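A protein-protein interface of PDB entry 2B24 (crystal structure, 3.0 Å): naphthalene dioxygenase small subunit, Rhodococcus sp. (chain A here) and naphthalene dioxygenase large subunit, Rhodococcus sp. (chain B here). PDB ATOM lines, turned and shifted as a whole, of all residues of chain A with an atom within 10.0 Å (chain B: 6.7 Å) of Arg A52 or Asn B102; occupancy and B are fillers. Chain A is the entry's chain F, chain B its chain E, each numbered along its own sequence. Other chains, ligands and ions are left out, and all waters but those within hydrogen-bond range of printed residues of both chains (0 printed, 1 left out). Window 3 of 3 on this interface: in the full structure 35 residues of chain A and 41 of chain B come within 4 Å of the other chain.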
ATOM      1  N   ILE A  48      15.406   9.738  21.676  1.00  0.00           N
ATOM      2  CA  ILE A  48      15.666   8.309  21.510  1.00  0.00           C
ATOM      3  C   ILE A  48      14.310   7.660  21.297  1.00  0.00           C
ATOM      4  O   ILE A  48      13.320   8.137  21.790  1.00  0.00           O
ATOM      5  CB  ILE A  48      16.372   7.698  22.755  1.00  0.00           C
ATOM      6  CG1 ILE A  48      17.813   8.172  22.894  1.00  0.00           C
ATOM      7  CG2 ILE A  48      16.382   6.192  22.688  1.00  0.00           C
ATOM      8  CD1 ILE A  48      18.425   7.870  24.245  1.00  0.00           C
ATOM      9  N   ARG A  49      14.270   6.579  20.549  1.00  0.00           N
ATOM     10  CA  ARG A  49      13.044   5.890  20.230  1.00  0.00           C
ATOM     11  C   ARG A  49      13.277   4.436  20.574  1.00  0.00           C
ATOM     12  O   ARG A  49      14.392   3.948  20.435  1.00  0.00           O
ATOM     13  CB  ARG A  49      12.818   5.982  18.736  1.00  0.00           C
ATOM     14  CG  ARG A  49      12.028   7.152  18.258  1.00  0.00           C
ATOM     15  CD  ARG A  49      10.725   6.711  17.694  1.00  0.00           C
ATOM     16  NE  ARG A  49      10.583   6.944  16.274  1.00  0.00           N
ATOM     17  CZ  ARG A  49       9.406   7.069  15.695  1.00  0.00           C
ATOM     18  NH1 ARG A  49       8.313   7.001  16.422  1.00  0.00           N
ATOM     19  NH2 ARG A  49       9.309   7.286  14.403  1.00  0.00           N
ATOM     20  N   VAL A  50      12.239   3.738  21.021  1.00  0.00           N
ATOM     21  CA  VAL A  50      12.316   2.300  21.269  1.00  0.00           C
ATOM     22  C   VAL A  50      11.079   1.667  20.668  1.00  0.00           C
ATOM     23  O   VAL A  50      10.058   2.320  20.577  1.00  0.00           O
ATOM     24  CB  VAL A  50      12.426   1.926  22.784  1.00  0.00           C
ATOM     25  CG1 VAL A  50      13.744   2.389  23.394  1.00  0.00           C
ATOM     26  CG2 VAL A  50      11.248   2.454  23.579  1.00  0.00           C
ATOM     27  N   THR A  51      11.184   0.412  20.232  1.00  0.00           N
ATOM     28  CA  THR A  51      10.036  -0.359  19.760  1.00  0.00           C
ATOM     29  C   THR A  51       9.116  -0.647  20.925  1.00  0.00           C
ATOM     30  O   THR A  51       9.525  -1.226  21.920  1.00  0.00           O
ATOM     31  CB  THR A  51      10.470  -1.675  19.165  1.00  0.00           C
ATOM     32  OG1 THR A  51      11.702  -1.492  18.490  1.00  0.00           O
ATOM     33  CG2 THR A  51       9.536  -2.089  18.071  1.00  0.00           C
ATOM     34  N   ARG A  52       7.876  -0.207  20.793  1.00  0.00           N
ATOM     35  CA  ARG A  52       6.839  -0.494  21.747  1.00  0.00           C
ATOM     36  C   ARG A  52       5.626  -0.861  20.914  1.00  0.00           C
ATOM     37  O   ARG A  52       5.638  -0.703  19.700  1.00  0.00           O
ATOM     38  CB  ARG A  52       6.552   0.732  22.616  1.00  0.00           C
ATOM     39  CG  ARG A  52       7.730   1.187  23.430  1.00  0.00           C
ATOM     40  CD  ARG A  52       7.412   1.567  24.857  1.00  0.00           C
ATOM     41  NE  ARG A  52       6.771   0.467  25.552  1.00  0.00           N
ATOM     42  CZ  ARG A  52       6.320   0.520  26.795  1.00  0.00           C
ATOM     43  NH1 ARG A  52       6.451   1.627  27.510  1.00  0.00           N
ATOM     44  NH2 ARG A  52       5.732  -0.545  27.324  1.00  0.00           N
ATOM     45  N   GLU A  53       4.580  -1.351  21.561  1.00  0.00           N
ATOM     46  CA  GLU A  53       3.365  -1.728  20.867  1.00  0.00           C
ATOM     47  C   GLU A  53       2.501  -0.500  20.562  1.00  0.00           C
ATOM     48  O   GLU A  53       2.662   0.546  21.197  1.00  0.00           O
ATOM     49  CB  GLU A  53       2.602  -2.747  21.706  1.00  0.00           C
ATOM     50  CG  GLU A  53       3.223  -2.979  23.058  1.00  0.00           C
ATOM     51  CD  GLU A  53       2.346  -2.473  24.177  1.00  0.00           C
ATOM     52  OE1 GLU A  53       2.841  -2.446  25.332  1.00  0.00           O
ATOM     53  OE2 GLU A  53       1.159  -2.124  23.913  1.00  0.00           O
ATOM     54  N   ARG A  54       1.594  -0.630  19.592  1.00  0.00           N
ATOM     55  CA  ARG A  54       0.619   0.415  19.284  1.00  0.00           C
ATOM     56  C   ARG A  54      -0.135   0.912  20.530  1.00  0.00           C
ATOM     57  O   ARG A  54      -0.248   2.118  20.756  1.00  0.00           O
ATOM     58  CB  ARG A  54      -0.372  -0.092  18.241  1.00  0.00           C
ATOM     59  CG  ARG A  54      -0.366   0.676  16.913  1.00  0.00           C
ATOM     60  CD  ARG A  54      -1.573   0.338  16.026  1.00  0.00           C
ATOM     61  NE  ARG A  54      -1.342   0.262  14.571  1.00  0.00           N
ATOM     62  CZ  ARG A  54      -0.781   1.210  13.822  1.00  0.00           C
ATOM     63  NH1 ARG A  54      -0.300   2.317  14.382  1.00  0.00           N
ATOM     64  NH2 ARG A  54      -0.679   1.037  12.506  1.00  0.00           N
ATOM     65  N   GLU A  55      -0.636  -0.025  21.336  1.00  0.00           N
ATOM     66  CA  GLU A  55      -1.330   0.275  22.593  1.00  0.00           C
ATOM     67  C   GLU A  55      -0.621   1.348  23.417  1.00  0.00           C
ATOM     68  O   GLU A  55      -1.218   2.391  23.710  1.00  0.00           O
ATOM     69  CB  GLU A  55      -1.494  -1.003  23.433  1.00  0.00           C
ATOM     70  CG  GLU A  55      -2.485  -0.900  24.592  1.00  0.00           C
ATOM     71  CD  GLU A  55      -2.450  -2.122  25.515  1.00  0.00           C
ATOM     72  OE1 GLU A  55      -3.347  -2.239  26.398  1.00  0.00           O
ATOM     73  OE2 GLU A  55      -1.517  -2.964  25.359  1.00  0.00           O
ATOM     74  N   ALA A  56       0.648   1.083  23.764  1.00  0.00           N
ATOM     75  CA  ALA A  56       1.465   1.909  24.681  1.00  0.00           C
ATOM     76  C   ALA A  56       1.384   3.381  24.352  1.00  0.00           C
ATOM     77  O   ALA A  56       1.277   3.743  23.185  1.00  0.00           O
ATOM     78  CB  ALA A  56       2.928   1.452  24.672  1.00  0.00           C
ATOM     79  N   VAL A  57       1.448   4.216  25.382  1.00  0.00           N
ATOM     80  CA  VAL A  57       1.273   5.666  25.242  1.00  0.00           C
ATOM     81  C   VAL A  57       2.141   6.322  24.166  1.00  0.00           C
ATOM     82  O   VAL A  57       1.648   7.130  23.391  1.00  0.00           O
ATOM     83  CB  VAL A  57       1.497   6.427  26.577  1.00  0.00           C
ATOM     84  CG1 VAL A  57       0.344   7.378  26.836  1.00  0.00           C
ATOM     85  CG2 VAL A  57       1.701   5.466  27.754  1.00  0.00           C
ATOM     86  N   THR A  58       3.424   5.968  24.123  1.00  0.00           N
ATOM     87  CA  THR A  58       4.393   6.638  23.262  1.00  0.00           C
ATOM     88  C   THR A  58       5.636   5.806  22.940  1.00  0.00           C
ATOM     89  O   THR A  58       5.980   4.853  23.628  1.00  0.00           O
ATOM     90  CB  THR A  58       4.803   7.991  23.886  1.00  0.00           C
ATOM     91  OG1 THR A  58       5.705   8.671  23.015  1.00  0.00           O
ATOM     92  CG2 THR A  58       5.634   7.789  25.138  1.00  0.00           C
ATOM     93  N   ASP A  59       6.321   6.224  21.887  1.00  0.00           N
ATOM     94  CA  ASP A  59       7.530   5.589  21.375  1.00  0.00           C
ATOM     95  C   ASP A  59       8.766   6.208  21.977  1.00  0.00           C
ATOM     96  O   ASP A  59       9.751   5.537  22.213  1.00  0.00           O
ATOM     97  CB  ASP A  59       7.593   5.837  19.875  1.00  0.00           C
ATOM     98  CG  ASP A  59       7.819   4.596  19.104  1.00  0.00           C
ATOM     99  OD1 ASP A  59       8.117   4.713  17.907  1.00  0.00           O
ATOM    100  OD2 ASP A  59       7.717   3.460  19.594  1.00  0.00           O
ATOM    101  N   VAL A  60       8.692   7.513  22.203  1.00  0.00           N
ATOM    102  CA  VAL A  60       9.836   8.346  22.505  1.00  0.00           C
ATOM    103  C   VAL A  60      10.221   8.237  23.967  1.00  0.00           C
ATOM    104  O   VAL A  60       9.397   8.431  24.853  1.00  0.00           O
ATOM    105  CB  VAL A  60       9.536   9.822  22.151  1.00  0.00           C
ATOM    106  CG1 VAL A  60      10.754  10.675  22.329  1.00  0.00           C
ATOM    107  CG2 VAL A  60       9.044   9.950  20.740  1.00  0.00           C
ATOM    108  N   VAL A  61      11.490   7.929  24.205  1.00  0.00           N
ATOM    109  CA  VAL A  61      12.084   7.879  25.541  1.00  0.00           C
ATOM    110  C   VAL A  61      12.088   9.263  26.225  1.00  0.00           C
ATOM    111  O   VAL A  61      12.522  10.243  25.618  1.00  0.00           O
ATOM    112  CB  VAL A  61      13.518   7.306  25.447  1.00  0.00           C
ATOM    113  CG1 VAL A  61      14.276   7.475  26.723  1.00  0.00           C
ATOM    114  CG2 VAL A  61      13.462   5.863  25.067  1.00  0.00           C
ATOM    115  N   GLU A  62      11.591   9.337  27.468  1.00  0.00           N
ATOM    116  CA  GLU A  62      11.698  10.560  28.276  1.00  0.00           C
ATOM    117  C   GLU A  62      12.874  10.527  29.235  1.00  0.00           C
ATOM    118  O   GLU A  62      13.138   9.523  29.872  1.00  0.00           O
ATOM    119  CB  GLU A  62      10.425  10.902  29.069  1.00  0.00           C
ATOM    120  CG  GLU A  62       9.248   9.944  28.962  1.00  0.00           C
ATOM    121  CD  GLU A  62       8.547   9.720  30.300  1.00  0.00           C
ATOM    122  OE1 GLU A  62       8.225   8.551  30.616  1.00  0.00           O
ATOM    123  OE2 GLU A  62       8.314  10.698  31.046  1.00  0.00           O
ATOM    124  N   THR A 161      15.141   3.214  15.888  1.00  0.00           N
ATOM    125  CA  THR A 161      15.515   3.061  17.271  1.00  0.00           C
ATOM    126  C   THR A 161      17.049   2.901  17.362  1.00  0.00           C
ATOM    127  O   THR A 161      17.708   3.758  17.956  1.00  0.00           O
ATOM    128  CB  THR A 161      14.714   1.938  17.898  1.00  0.00           C
ATOM    129  OG1 THR A 161      14.829   0.762  17.102  1.00  0.00           O
ATOM    130  CG2 THR A 161      13.275   2.251  17.755  1.00  0.00           C
ATOM    131  N   GLU B  57       9.296  -1.984  38.804  1.00  0.00           N
ATOM    132  CA  GLU B  57       8.051  -2.630  39.215  1.00  0.00           C
ATOM    133  C   GLU B  57       7.855  -3.992  38.553  1.00  0.00           C
ATOM    134  O   GLU B  57       8.663  -4.406  37.721  1.00  0.00           O
ATOM    135  CB  GLU B  57       6.814  -1.744  38.967  1.00  0.00           C
ATOM    136  CG  GLU B  57       7.047  -0.247  38.817  1.00  0.00           C
ATOM    137  CD  GLU B  57       7.101   0.525  40.140  1.00  0.00           C
ATOM    138  OE1 GLU B  57       7.509  -0.037  41.188  1.00  0.00           O
ATOM    139  OE2 GLU B  57       6.755   1.732  40.120  1.00  0.00           O
ATOM    140  N   ARG B  58       6.775  -4.680  38.935  1.00  0.00           N
ATOM    141  CA  ARG B  58       6.478  -6.026  38.458  1.00  0.00           C
ATOM    142  C   ARG B  58       5.896  -5.982  37.064  1.00  0.00           C
ATOM    143  O   ARG B  58       4.914  -5.296  36.826  1.00  0.00           O
ATOM    144  CB  ARG B  58       5.501  -6.747  39.397  1.00  0.00           C
ATOM    145  CG  ARG B  58       5.765  -6.588  40.897  1.00  0.00           C
ATOM    146  CD  ARG B  58       6.556  -7.722  41.509  1.00  0.00           C
ATOM    147  NE  ARG B  58       5.750  -8.591  42.372  1.00  0.00           N
ATOM    148  CZ  ARG B  58       5.780  -8.585  43.714  1.00  0.00           C
ATOM    149  NH1 ARG B  58       6.568  -7.737  44.377  1.00  0.00           N
ATOM    150  NH2 ARG B  58       5.009  -9.426  44.398  1.00  0.00           N
ATOM    151  N   GLY B  59       6.509  -6.732  36.151  1.00  0.00           N
ATOM    152  CA  GLY B  59       6.110  -6.765  34.751  1.00  0.00           C
ATOM    153  C   GLY B  59       7.105  -6.115  33.794  1.00  0.00           C
ATOM    154  O   GLY B  59       7.292  -6.597  32.689  1.00  0.00           O
ATOM    155  N   ASP B  60       7.731  -5.024  34.235  1.00  0.00           N
ATOM    156  CA  ASP B  60       8.759  -4.295  33.496  1.00  0.00           C
ATOM    157  C   ASP B  60       9.812  -5.203  32.916  1.00  0.00           C
ATOM    158  O   ASP B  60      10.383  -5.992  33.622  1.00  0.00           O
ATOM    159  CB  ASP B  60       9.444  -3.281  34.412  1.00  0.00           C
ATOM    160  CG  ASP B  60       8.542  -2.130  34.793  1.00  0.00           C
ATOM    161  OD1 ASP B  60       7.365  -2.115  34.396  1.00  0.00           O
ATOM    162  OD2 ASP B  60       8.928  -1.183  35.493  1.00  0.00           O
ATOM    163  N   TYR B  61      10.064  -5.080  31.620  1.00  0.00           N
ATOM    164  CA  TYR B  61      11.070  -5.889  30.948  1.00  0.00           C
ATOM    165  C   TYR B  61      11.861  -5.059  29.985  1.00  0.00           C
ATOM    166  O   TYR B  61      11.412  -3.998  29.547  1.00  0.00           O
ATOM    167  CB  TYR B  61      10.448  -7.067  30.189  1.00  0.00           C
ATOM    168  CG  TYR B  61       9.587  -6.685  29.009  1.00  0.00           C
ATOM    169  CD1 TYR B  61      10.132  -6.569  27.738  1.00  0.00           C
ATOM    170  CD2 TYR B  61       8.220  -6.450  29.162  1.00  0.00           C
ATOM    171  CE1 TYR B  61       9.346  -6.205  26.666  1.00  0.00           C
ATOM    172  CE2 TYR B  61       7.445  -6.091  28.101  1.00  0.00           C
ATOM    173  CZ  TYR B  61       8.011  -5.975  26.860  1.00  0.00           C
ATOM    174  OH  TYR B  61       7.227  -5.637  25.807  1.00  0.00           O
ATOM    175  N   ARG B  75      11.200  -8.385  35.516  1.00  0.00           N
ATOM    176  CA  ARG B  75      10.882  -8.613  36.916  1.00  0.00           C
ATOM    177  C   ARG B  75       9.520  -9.284  36.988  1.00  0.00           C
ATOM    178  O   ARG B  75       8.503  -8.604  36.875  1.00  0.00           O
ATOM    179  CB  ARG B  75      10.856  -7.282  37.682  1.00  0.00           C
ATOM    180  CG  ARG B  75      11.045  -7.425  39.186  1.00  0.00           C
ATOM    181  CD  ARG B  75      11.083  -6.126  39.977  1.00  0.00           C
ATOM    182  NE  ARG B  75      12.384  -5.463  39.866  1.00  0.00           N
ATOM    183  CZ  ARG B  75      13.485  -5.862  40.481  1.00  0.00           C
ATOM    184  NH1 ARG B  75      13.452  -6.913  41.273  1.00  0.00           N
ATOM    185  NH2 ARG B  75      14.624  -5.211  40.311  1.00  0.00           N
ATOM    186  N   ARG B  97       8.216  -8.656  20.841  1.00  0.00           N
ATOM    187  CA  ARG B  97       8.837  -7.894  19.752  1.00  0.00           C
ATOM    188  C   ARG B  97       9.090  -6.396  20.023  1.00  0.00           C
ATOM    189  O   ARG B  97       9.509  -5.660  19.133  1.00  0.00           O
ATOM    190  CB  ARG B  97       8.065  -8.079  18.449  1.00  0.00           C
ATOM    191  CG  ARG B  97       8.454  -9.318  17.677  1.00  0.00           C
ATOM    192  CD  ARG B  97       7.429  -9.761  16.663  1.00  0.00           C
ATOM    193  NE  ARG B  97       6.060  -9.657  17.158  1.00  0.00           N
ATOM    194  CZ  ARG B  97       5.094  -9.026  16.532  1.00  0.00           C
ATOM    195  NH1 ARG B  97       5.318  -8.447  15.373  1.00  0.00           N
ATOM    196  NH2 ARG B  97       3.893  -8.974  17.058  1.00  0.00           N
ATOM    197  N   ALA B  98       8.831  -5.949  21.245  1.00  0.00           N
ATOM    198  CA  ALA B  98       9.236  -4.628  21.698  1.00  0.00           C
ATOM    199  C   ALA B  98      10.655  -4.734  22.222  1.00  0.00           C
ATOM    200  O   ALA B  98      11.221  -5.827  22.213  1.00  0.00           O
ATOM    201  CB  ALA B  98       8.321  -4.166  22.772  1.00  0.00           C
ATOM    202  N   GLU B  99      11.244  -3.613  22.650  1.00  0.00           N
ATOM    203  CA  GLU B  99      12.569  -3.625  23.285  1.00  0.00           C
ATOM    204  C   GLU B  99      12.475  -3.274  24.751  1.00  0.00           C
ATOM    205  O   GLU B  99      13.394  -3.508  25.509  1.00  0.00           O
ATOM    206  CB  GLU B  99      13.532  -2.655  22.629  1.00  0.00           C
ATOM    207  CG  GLU B  99      13.175  -2.244  21.223  1.00  0.00           C
ATOM    208  CD  GLU B  99      14.119  -1.222  20.644  1.00  0.00           C
ATOM    209  OE1 GLU B  99      15.056  -0.807  21.335  1.00  0.00           O
ATOM    210  OE2 GLU B  99      13.916  -0.842  19.491  1.00  0.00           O
ATOM    211  N   MET B 100      11.348  -2.695  25.134  1.00  0.00           N
ATOM    212  CA  MET B 100      11.087  -2.268  26.486  1.00  0.00           C
ATOM    213  C   MET B 100       9.603  -2.348  26.685  1.00  0.00           C
ATOM    214  O   MET B 100       8.829  -2.237  25.726  1.00  0.00           O
ATOM    215  CB  MET B 100      11.488  -0.812  26.649  1.00  0.00           C
ATOM    216  CG  MET B 100      12.961  -0.616  26.831  1.00  0.00           C
ATOM    217  SD  MET B 100      13.397   1.038  27.080  1.00  0.00           S
ATOM    218  CE  MET B 100      11.940   1.654  27.820  1.00  0.00           C
ATOM    219  N   GLY B 101       9.192  -2.514  27.938  1.00  0.00           N
ATOM    220  CA  GLY B 101       7.787  -2.395  28.264  1.00  0.00           C
ATOM    221  C   GLY B 101       7.425  -2.903  29.621  1.00  0.00           C
ATOM    222  O   GLY B 101       8.300  -3.116  30.439  1.00  0.00           O
ATOM    223  N   ASN B 102       6.122  -3.070  29.835  1.00  0.00           N
ATOM    224  CA  ASN B 102       5.576  -3.703  31.016  1.00  0.00           C
ATOM    225  C   ASN B 102       4.406  -4.586  30.629  1.00  0.00           C
ATOM    226  O   ASN B 102       3.402  -4.095  30.107  1.00  0.00           O
ATOM    227  CB  ASN B 102       5.115  -2.668  32.039  1.00  0.00           C
ATOM    228  CG  ASN B 102       4.483  -3.310  33.264  1.00  0.00           C
ATOM    229  OD1 ASN B 102       3.293  -3.634  33.278  1.00  0.00           O
ATOM    230  ND2 ASN B 102       5.289  -3.514  34.293  1.00  0.00           N
ATOM    231  N   THR B 103       4.535  -5.884  30.893  1.00  0.00           N
ATOM    232  CA  THR B 103       3.469  -6.839  30.632  1.00  0.00           C
ATOM    233  C   THR B 103       3.444  -7.912  31.706  1.00  0.00           C
ATOM    234  O   THR B 103       4.485  -8.267  32.253  1.00  0.00           O
ATOM    235  CB  THR B 103       3.641  -7.460  29.238  1.00  0.00           C
ATOM    236  OG1 THR B 103       2.568  -8.354  28.980  1.00  0.00           O
ATOM    237  CG2 THR B 103       4.806  -8.382  29.199  1.00  0.00           C
ATOM    238  N   SER B 104       2.253  -8.416  32.022  1.00  0.00           N
ATOM    239  CA  SER B 104       2.131  -9.547  32.932  1.00  0.00           C
ATOM    240  C   SER B 104       2.440 -10.850  32.202  1.00  0.00           C
ATOM    241  O   SER B 104       3.207 -11.664  32.680  1.00  0.00           O
ATOM    242  CB  SER B 104       0.745  -9.580  33.584  1.00  0.00           C
ATOM    243  OG  SER B 104      -0.303  -9.705  32.638  1.00  0.00           O
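Glu B99 touches Val A50 (OE2 to CA, 3.9 Å). Met B100 touches Val A50. CG2 of Thr A51 touches O of Arg B97, 3.7 Å away. O of Thr A51 touches CB of Ala B98, at 3.3 Å. Thr A51 touches Met B100 (O to N, 3.98 Å). NH2 of Arg A52 touches CA of Gly B101 (2.9 Å). Arg A52 touches Asn B102.
Of the 14 printed residues of chain B, 6 touch a printed residue of chain A. Printed residues of chain B that touch a printed residue of chain A: Arg B97, Ala B98, Glu B99, Met B100, Gly B101 and Asn B102. Printed residues of chain A that touch a printed residue of chain B: Val A50, Thr A51, Arg A52 and Thr A161. Hydrophobic or aromatic side chains of chain A within 4 Å of the printed part of chain B: Val A50.
The side-chain carboxylate (OE2) of Glu B99 is in hydrogen-bond range of the side-chain hydroxyl (OG1) of Thr A161 (3.0 Å). OG1 of Thr A51 is in hydrogen-bond range of OE2 of Glu B99, 2.5 Å away. The guanidinium group (NE) of Arg A52 lies within hydrogen-bond range of the backbone carbonyl oxygen (O) of Met B100, at 3.4 Å.
Of the printed residues of chain B, Thr A51 touches Arg B97, Ala B98, Glu B99 and Met B100. Printed residues of chain B within 4 Å of Arg A52: Met B100, Gly B101 and Asn B102. Glu A62 touches none of the printed residues of chain B. Arg B58 touches none of the printed residues of chain A. No residue of chain A comes within 4 Å of Gly B59. No residue of chain A comes within 4 Å of Asp B60. Of the printed residues of chain A, Ala B98 touches Thr A51. Printed residues of chain A within 4 Å of Met B100: Val A50 (3.9 Å), Thr A51 (3.98 Å) and Arg A52 (3.4 Å). Gly B101 touches one residue of chain A. The nearest printed residue of chain B that does not touch Thr A161 is Arg B97 (8.6 Å).
ND2 of Asn B102 is in hydrogen-bond range of O of Arg B58 (3.1 Å). The guanidinium group (NH2) of Arg A52 is in salt-bridge range of the side-chain carboxylate (OE1) of Glu A53 (3.99 Å). The backbone NH (N) of Tyr B61 sits at hydrogen-bond distance from the backbone carbonyl oxygen (O) of Gly B101. The side-chain carboxylate (OD1) of Asp B60 sits at hydrogen-bond distance from the side-chain amide nitrogen (ND2) of Asn B102, at 2.5 Å. The backbone NH (N) of Val A50 sits at hydrogen-bond distance from the backbone carbonyl oxygen (O) of Asp A59 (3.3 Å).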
